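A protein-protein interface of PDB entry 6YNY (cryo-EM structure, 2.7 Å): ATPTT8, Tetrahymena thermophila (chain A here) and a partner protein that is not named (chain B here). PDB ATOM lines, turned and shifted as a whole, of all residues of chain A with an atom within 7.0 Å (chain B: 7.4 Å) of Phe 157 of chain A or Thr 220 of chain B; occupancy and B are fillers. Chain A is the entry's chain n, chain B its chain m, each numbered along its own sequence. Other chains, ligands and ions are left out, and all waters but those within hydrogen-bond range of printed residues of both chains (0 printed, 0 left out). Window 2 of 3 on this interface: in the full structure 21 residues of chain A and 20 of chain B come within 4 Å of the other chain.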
ATOM      1  N   GLY A 152     -21.488  11.715  -5.645  1.00  0.00           N
ATOM      2  CA  GLY A 152     -22.317  12.213  -4.564  1.00  0.00           C
ATOM      3  C   GLY A 152     -21.763  11.858  -3.199  1.00  0.00           C
ATOM      4  O   GLY A 152     -21.778  12.679  -2.280  1.00  0.00           O
ATOM      5  N   ILE A 153     -21.268  10.631  -3.047  1.00  0.00           N
ATOM      6  CA  ILE A 153     -20.653  10.232  -1.789  1.00  0.00           C
ATOM      7  C   ILE A 153     -19.348  10.981  -1.577  1.00  0.00           C
ATOM      8  O   ILE A 153     -19.044  11.426  -0.464  1.00  0.00           O
ATOM      9  CB  ILE A 153     -20.441   8.710  -1.765  1.00  0.00           C
ATOM     10  CG1 ILE A 153     -21.787   7.989  -1.743  1.00  0.00           C
ATOM     11  CG2 ILE A 153     -19.620   8.324  -0.569  1.00  0.00           C
ATOM     12  CD1 ILE A 153     -21.716   6.541  -2.149  1.00  0.00           C
ATOM     13  N   GLN A 154     -18.553  11.129  -2.634  1.00  0.00           N
ATOM     14  CA  GLN A 154     -17.319  11.895  -2.528  1.00  0.00           C
ATOM     15  C   GLN A 154     -17.603  13.359  -2.224  1.00  0.00           C
ATOM     16  O   GLN A 154     -16.784  14.034  -1.595  1.00  0.00           O
ATOM     17  CB  GLN A 154     -16.520  11.752  -3.821  1.00  0.00           C
ATOM     18  CG  GLN A 154     -15.106  12.264  -3.750  1.00  0.00           C
ATOM     19  CD  GLN A 154     -14.328  11.974  -5.007  1.00  0.00           C
ATOM     20  OE1 GLN A 154     -14.893  11.570  -6.022  1.00  0.00           O
ATOM     21  NE2 GLN A 154     -13.023  12.167  -4.946  1.00  0.00           N
ATOM     22  N   LYS A 155     -18.754  13.865  -2.665  1.00  0.00           N
ATOM     23  CA  LYS A 155     -19.148  15.229  -2.337  1.00  0.00           C
ATOM     24  C   LYS A 155     -19.596  15.352  -0.890  1.00  0.00           C
ATOM     25  O   LYS A 155     -19.491  16.430  -0.296  1.00  0.00           O
ATOM     26  CB  LYS A 155     -20.273  15.682  -3.261  1.00  0.00           C
ATOM     27  CG  LYS A 155     -19.815  16.464  -4.451  1.00  0.00           C
ATOM     28  CD  LYS A 155     -19.491  17.882  -4.065  1.00  0.00           C
ATOM     29  CE  LYS A 155     -19.042  18.677  -5.261  1.00  0.00           C
ATOM     30  NZ  LYS A 155     -18.720  20.068  -4.903  1.00  0.00           N
ATOM     31  N   LYS A 156     -20.103  14.265  -0.315  1.00  0.00           N
ATOM     32  CA  LYS A 156     -20.618  14.296   1.046  1.00  0.00           C
ATOM     33  C   LYS A 156     -19.505  14.163   2.073  1.00  0.00           C
ATOM     34  O   LYS A 156     -19.486  14.893   3.069  1.00  0.00           O
ATOM     35  CB  LYS A 156     -21.638  13.176   1.226  1.00  0.00           C
ATOM     36  CG  LYS A 156     -22.346  13.155   2.557  1.00  0.00           C
ATOM     37  CD  LYS A 156     -23.367  12.040   2.584  1.00  0.00           C
ATOM     38  CE  LYS A 156     -24.081  11.945   3.912  1.00  0.00           C
ATOM     39  NZ  LYS A 156     -24.894  13.141   4.202  1.00  0.00           N
ATOM     40  N   PHE A 157     -18.562  13.253   1.838  1.00  0.00           N
ATOM     41  CA  PHE A 157     -17.509  12.962   2.795  1.00  0.00           C
ATOM     42  C   PHE A 157     -16.145  13.504   2.404  1.00  0.00           C
ATOM     43  O   PHE A 157     -15.263  13.568   3.264  1.00  0.00           O
ATOM     44  CB  PHE A 157     -17.399  11.448   2.997  1.00  0.00           C
ATOM     45  CG  PHE A 157     -18.636  10.826   3.562  1.00  0.00           C
ATOM     46  CD1 PHE A 157     -18.860  10.812   4.921  1.00  0.00           C
ATOM     47  CD2 PHE A 157     -19.578  10.255   2.730  1.00  0.00           C
ATOM     48  CE1 PHE A 157     -19.995  10.242   5.438  1.00  0.00           C
ATOM     49  CE2 PHE A 157     -20.712   9.686   3.246  1.00  0.00           C
ATOM     50  CZ  PHE A 157     -20.920   9.679   4.600  1.00  0.00           C
ATOM     51  N   PHE A 158     -15.948  13.890   1.148  1.00  0.00           N
ATOM     52  CA  PHE A 158     -14.687  14.469   0.687  1.00  0.00           C
ATOM     53  C   PHE A 158     -14.959  15.753  -0.086  1.00  0.00           C
ATOM     54  O   PHE A 158     -14.548  15.900  -1.239  1.00  0.00           O
ATOM     55  CB  PHE A 158     -13.918  13.479  -0.181  1.00  0.00           C
ATOM     56  CG  PHE A 158     -13.708  12.140   0.450  1.00  0.00           C
ATOM     57  CD1 PHE A 158     -12.524  11.842   1.091  1.00  0.00           C
ATOM     58  CD2 PHE A 158     -14.684  11.170   0.383  1.00  0.00           C
ATOM     59  CE1 PHE A 158     -12.325  10.608   1.657  1.00  0.00           C
ATOM     60  CE2 PHE A 158     -14.487   9.935   0.952  1.00  0.00           C
ATOM     61  CZ  PHE A 158     -13.307   9.656   1.586  1.00  0.00           C
ATOM     62  N   PRO A 159     -15.650  16.714   0.527  1.00  0.00           N
ATOM     63  CA  PRO A 159     -15.893  17.986  -0.163  1.00  0.00           C
ATOM     64  C   PRO A 159     -14.630  18.786  -0.397  1.00  0.00           C
ATOM     65  O   PRO A 159     -14.606  19.632  -1.298  1.00  0.00           O
ATOM     66  CB  PRO A 159     -16.854  18.715   0.779  1.00  0.00           C
ATOM     67  CG  PRO A 159     -16.578  18.133   2.107  1.00  0.00           C
ATOM     68  CD  PRO A 159     -16.217  16.711   1.883  1.00  0.00           C
ATOM     69  N   GLU A 160     -13.582  18.538   0.386  1.00  0.00           N
ATOM     70  CA  GLU A 160     -12.307  19.221   0.231  1.00  0.00           C
ATOM     71  C   GLU A 160     -11.550  18.790  -1.018  1.00  0.00           C
ATOM     72  O   GLU A 160     -10.516  19.390  -1.330  1.00  0.00           O
ATOM     73  CB  GLU A 160     -11.443  18.982   1.469  1.00  0.00           C
ATOM     74  CG  GLU A 160     -11.185  17.513   1.801  1.00  0.00           C
ATOM     75  CD  GLU A 160     -12.269  16.898   2.659  1.00  0.00           C
ATOM     76  OE1 GLU A 160     -13.304  17.561   2.876  1.00  0.00           O
ATOM     77  OE2 GLU A 160     -12.088  15.752   3.117  1.00  0.00           O
ATOM     78  N   HIS A 161     -12.029  17.774  -1.733  1.00  0.00           N
ATOM     79  CA  HIS A 161     -11.356  17.310  -2.935  1.00  0.00           C
ATOM     80  C   HIS A 161     -11.686  18.147  -4.159  1.00  0.00           C
ATOM     81  O   HIS A 161     -10.912  18.144  -5.121  1.00  0.00           O
ATOM     82  CB  HIS A 161     -11.735  15.857  -3.223  1.00  0.00           C
ATOM     83  CG  HIS A 161     -11.094  14.865  -2.309  1.00  0.00           C
ATOM     84  ND1 HIS A 161     -11.301  13.509  -2.432  1.00  0.00           N
ATOM     85  CD2 HIS A 161     -10.248  15.024  -1.265  1.00  0.00           C
ATOM     86  CE1 HIS A 161     -10.611  12.876  -1.502  1.00  0.00           C
ATOM     87  NE2 HIS A 161      -9.964  13.773  -0.779  1.00  0.00           N
ATOM     88  N   ASP B   2     -26.215  11.447  -5.634  1.00  0.00           N
ATOM     89  CA  ASP B   2     -26.477  10.184  -4.968  1.00  0.00           C
ATOM     90  C   ASP B   2     -27.951  10.088  -4.584  1.00  0.00           C
ATOM     91  O   ASP B   2     -28.702  11.062  -4.640  1.00  0.00           O
ATOM     92  CB  ASP B   2     -25.584  10.032  -3.738  1.00  0.00           C
ATOM     93  CG  ASP B   2     -25.706  11.199  -2.783  1.00  0.00           C
ATOM     94  OD1 ASP B   2     -25.958  12.326  -3.257  1.00  0.00           O
ATOM     95  OD2 ASP B   2     -25.550  10.990  -1.562  1.00  0.00           O
ATOM     96  N   GLU B  40     -31.441   8.965   4.446  1.00  0.00           N
ATOM     97  CA  GLU B  40     -30.018   8.685   4.591  1.00  0.00           C
ATOM     98  C   GLU B  40     -29.683   8.262   6.013  1.00  0.00           C
ATOM     99  O   GLU B  40     -28.863   7.362   6.222  1.00  0.00           O
ATOM    100  CB  GLU B  40     -29.200   9.912   4.201  1.00  0.00           C
ATOM    101  CG  GLU B  40     -29.035  10.100   2.710  1.00  0.00           C
ATOM    102  CD  GLU B  40     -28.265  11.359   2.366  1.00  0.00           C
ATOM    103  OE1 GLU B  40     -28.117  12.230   3.247  1.00  0.00           O
ATOM    104  OE2 GLU B  40     -27.799  11.476   1.214  1.00  0.00           O
ATOM    105  N   THR B  43     -30.743   4.652   6.960  1.00  0.00           N
ATOM    106  CA  THR B  43     -29.865   3.635   6.400  1.00  0.00           C
ATOM    107  C   THR B  43     -28.563   3.478   7.168  1.00  0.00           C
ATOM    108  O   THR B  43     -27.780   2.579   6.844  1.00  0.00           O
ATOM    109  CB  THR B  43     -29.562   3.969   4.943  1.00  0.00           C
ATOM    110  OG1 THR B  43     -29.103   5.322   4.845  1.00  0.00           O
ATOM    111  CG2 THR B  43     -30.798   3.803   4.110  1.00  0.00           C
ATOM    112  N   LYS B  44     -28.311   4.318   8.172  1.00  0.00           N
ATOM    113  CA  LYS B  44     -27.093   4.251   8.968  1.00  0.00           C
ATOM    114  C   LYS B  44     -27.362   3.774  10.388  1.00  0.00           C
ATOM    115  O   LYS B  44     -26.571   4.052  11.293  1.00  0.00           O
ATOM    116  CB  LYS B  44     -26.412   5.618   8.988  1.00  0.00           C
ATOM    117  CG  LYS B  44     -25.929   6.072   7.631  1.00  0.00           C
ATOM    118  CD  LYS B  44     -25.627   7.542   7.620  1.00  0.00           C
ATOM    119  CE  LYS B  44     -25.285   8.020   6.223  1.00  0.00           C
ATOM    120  NZ  LYS B  44     -25.182   9.508   6.159  1.00  0.00           N
ATOM    121  N   PHE B 214     -19.925   5.630  16.402  1.00  0.00           N
ATOM    122  CA  PHE B 214     -19.102   4.861  15.486  1.00  0.00           C
ATOM    123  C   PHE B 214     -18.713   3.530  16.106  1.00  0.00           C
ATOM    124  O   PHE B 214     -18.315   3.462  17.272  1.00  0.00           O
ATOM    125  CB  PHE B 214     -17.839   5.635  15.113  1.00  0.00           C
ATOM    126  CG  PHE B 214     -16.871   4.842  14.288  1.00  0.00           C
ATOM    127  CD1 PHE B 214     -16.988   4.798  12.915  1.00  0.00           C
ATOM    128  CD2 PHE B 214     -15.848   4.136  14.888  1.00  0.00           C
ATOM    129  CE1 PHE B 214     -16.101   4.064  12.159  1.00  0.00           C
ATOM    130  CE2 PHE B 214     -14.966   3.405  14.138  1.00  0.00           C
ATOM    131  CZ  PHE B 214     -15.091   3.369  12.772  1.00  0.00           C
ATOM    132  N   HIS B 215     -18.830   2.468  15.312  1.00  0.00           N
ATOM    133  CA  HIS B 215     -18.258   1.187  15.646  1.00  0.00           C
ATOM    134  C   HIS B 215     -17.744   0.566  14.355  1.00  0.00           C
ATOM    135  O   HIS B 215     -18.362   0.735  13.293  1.00  0.00           O
ATOM    136  CB  HIS B 215     -19.260   0.249  16.334  1.00  0.00           C
ATOM    137  CG  HIS B 215     -20.494  -0.027  15.539  1.00  0.00           C
ATOM    138  ND1 HIS B 215     -20.733  -1.244  14.940  1.00  0.00           N
ATOM    139  CD2 HIS B 215     -21.569   0.746  15.264  1.00  0.00           C
ATOM    140  CE1 HIS B 215     -21.898  -1.205  14.320  1.00  0.00           C
ATOM    141  NE2 HIS B 215     -22.426  -0.008  14.499  1.00  0.00           N
ATOM    142  N   GLY B 218     -20.023  -0.681  11.623  1.00  0.00           N
ATOM    143  CA  GLY B 218     -21.156   0.186  11.402  1.00  0.00           C
ATOM    144  C   GLY B 218     -21.248   0.688   9.973  1.00  0.00           C
ATOM    145  O   GLY B 218     -20.579   0.207   9.058  1.00  0.00           O
ATOM    146  N   GLN B 219     -22.100   1.692   9.795  1.00  0.00           N
ATOM    147  CA  GLN B 219     -22.442   2.225   8.485  1.00  0.00           C
ATOM    148  C   GLN B 219     -21.915   3.645   8.357  1.00  0.00           C
ATOM    149  O   GLN B 219     -22.199   4.498   9.204  1.00  0.00           O
ATOM    150  CB  GLN B 219     -23.955   2.219   8.273  1.00  0.00           C
ATOM    151  CG  GLN B 219     -24.598   0.856   8.369  1.00  0.00           C
ATOM    152  CD  GLN B 219     -24.299  -0.016   7.179  1.00  0.00           C
ATOM    153  OE1 GLN B 219     -24.130   0.472   6.063  1.00  0.00           O
ATOM    154  NE2 GLN B 219     -24.231  -1.316   7.408  1.00  0.00           N
ATOM    155  N   THR B 220     -21.149   3.893   7.299  1.00  0.00           N
ATOM    156  CA  THR B 220     -20.676   5.228   6.970  1.00  0.00           C
ATOM    157  C   THR B 220     -21.153   5.687   5.602  1.00  0.00           C
ATOM    158  O   THR B 220     -21.714   6.781   5.481  1.00  0.00           O
ATOM    159  CB  THR B 220     -19.144   5.278   7.031  1.00  0.00           C
ATOM    160  OG1 THR B 220     -18.705   5.048   8.375  1.00  0.00           O
ATOM    161  CG2 THR B 220     -18.645   6.621   6.566  1.00  0.00           C
ATOM    162  N   PHE B 221     -20.951   4.877   4.568  1.00  0.00           N
ATOM    163  CA  PHE B 221     -21.456   5.189   3.240  1.00  0.00           C
ATOM    164  C   PHE B 221     -22.838   4.577   3.039  1.00  0.00           C
ATOM    165  O   PHE B 221     -23.649   5.092   2.268  1.00  0.00           O
ATOM    166  CB  PHE B 221     -20.497   4.678   2.163  1.00  0.00           C
ATOM    167  CG  PHE B 221     -19.134   5.306   2.205  1.00  0.00           C
ATOM    168  CD1 PHE B 221     -18.037   4.615   1.733  1.00  0.00           C
ATOM    169  CD2 PHE B 221     -18.946   6.581   2.707  1.00  0.00           C
ATOM    170  CE1 PHE B 221     -16.782   5.180   1.761  1.00  0.00           C
ATOM    171  CE2 PHE B 221     -17.693   7.147   2.737  1.00  0.00           C
ATOM    172  CZ  PHE B 221     -16.611   6.446   2.263  1.00  0.00           C
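The side-chain carboxylate of Glu 40 of chain B lies within salt-bridge range of the side-chain amino group of Lys 156 of chain A, 3.5 Å away.
The side-chain hydroxyl of Thr 43 of chain B is in hydrogen-bond range of the backbone carbonyl oxygen of Glu 40 of chain B (2.5 Å).
Among the printed residues, pairs that only touch across the chains: Phe 157 of chain A with Thr 220 of chain B (3.1 Å), Lys 156 of chain A with Lys 44 of chain B (3.5 Å), Phe 157 of chain A with Phe 221 of chain B (3.6 Å), Ile 153 of chain A with Phe 221 of chain B (3.8 Å) and Gly 152 of chain A with Asp 2 of chain B (3.9 Å).
Printed residues of chain B within 4 Å of Phe 157 of chain A: Thr 220 and Phe 221. Thr 220 of chain B touches one residue of chain A. Printed residues of chain B within 4 Å of Gly 152 of chain A: Asp 2 (3.9 Å). Of the printed residues of chain B, Ile 153 of chain A touches Phe 221 (3.8 Å). Printed residues of chain A within 4 Å of Phe 221 of chain B: Ile 153 (3.8 Å) and Phe 157 (3.6 Å). Of the printed residues of chain B, Lys 156 of chain A touches Glu 40 (3.5 Å) and Lys 44 (3.5 Å). Of the printed residues of chain A, Glu 40 of chain B touches Lys 156. Gln 219 of chain B touches none of the printed residues of chain A. Phe 214 of chain B touches none of the printed residues of chain A. The nearest printed residue of chain B that does not touch Ile 153 of chain A is Asp 2 of chain B (4.4 Å).
Hydrophobic or aromatic side chains of chain B within 4 Å of the printed part of chain A: Phe 221. Among the printed residues, 6 pairs touch across the chains. Among the printed residues, Asp or Glu carboxylates within 4 Å of a Lys or Arg side-chain nitrogen of the other chain: Lys 156 of chain A with Glu 40 of chain B.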
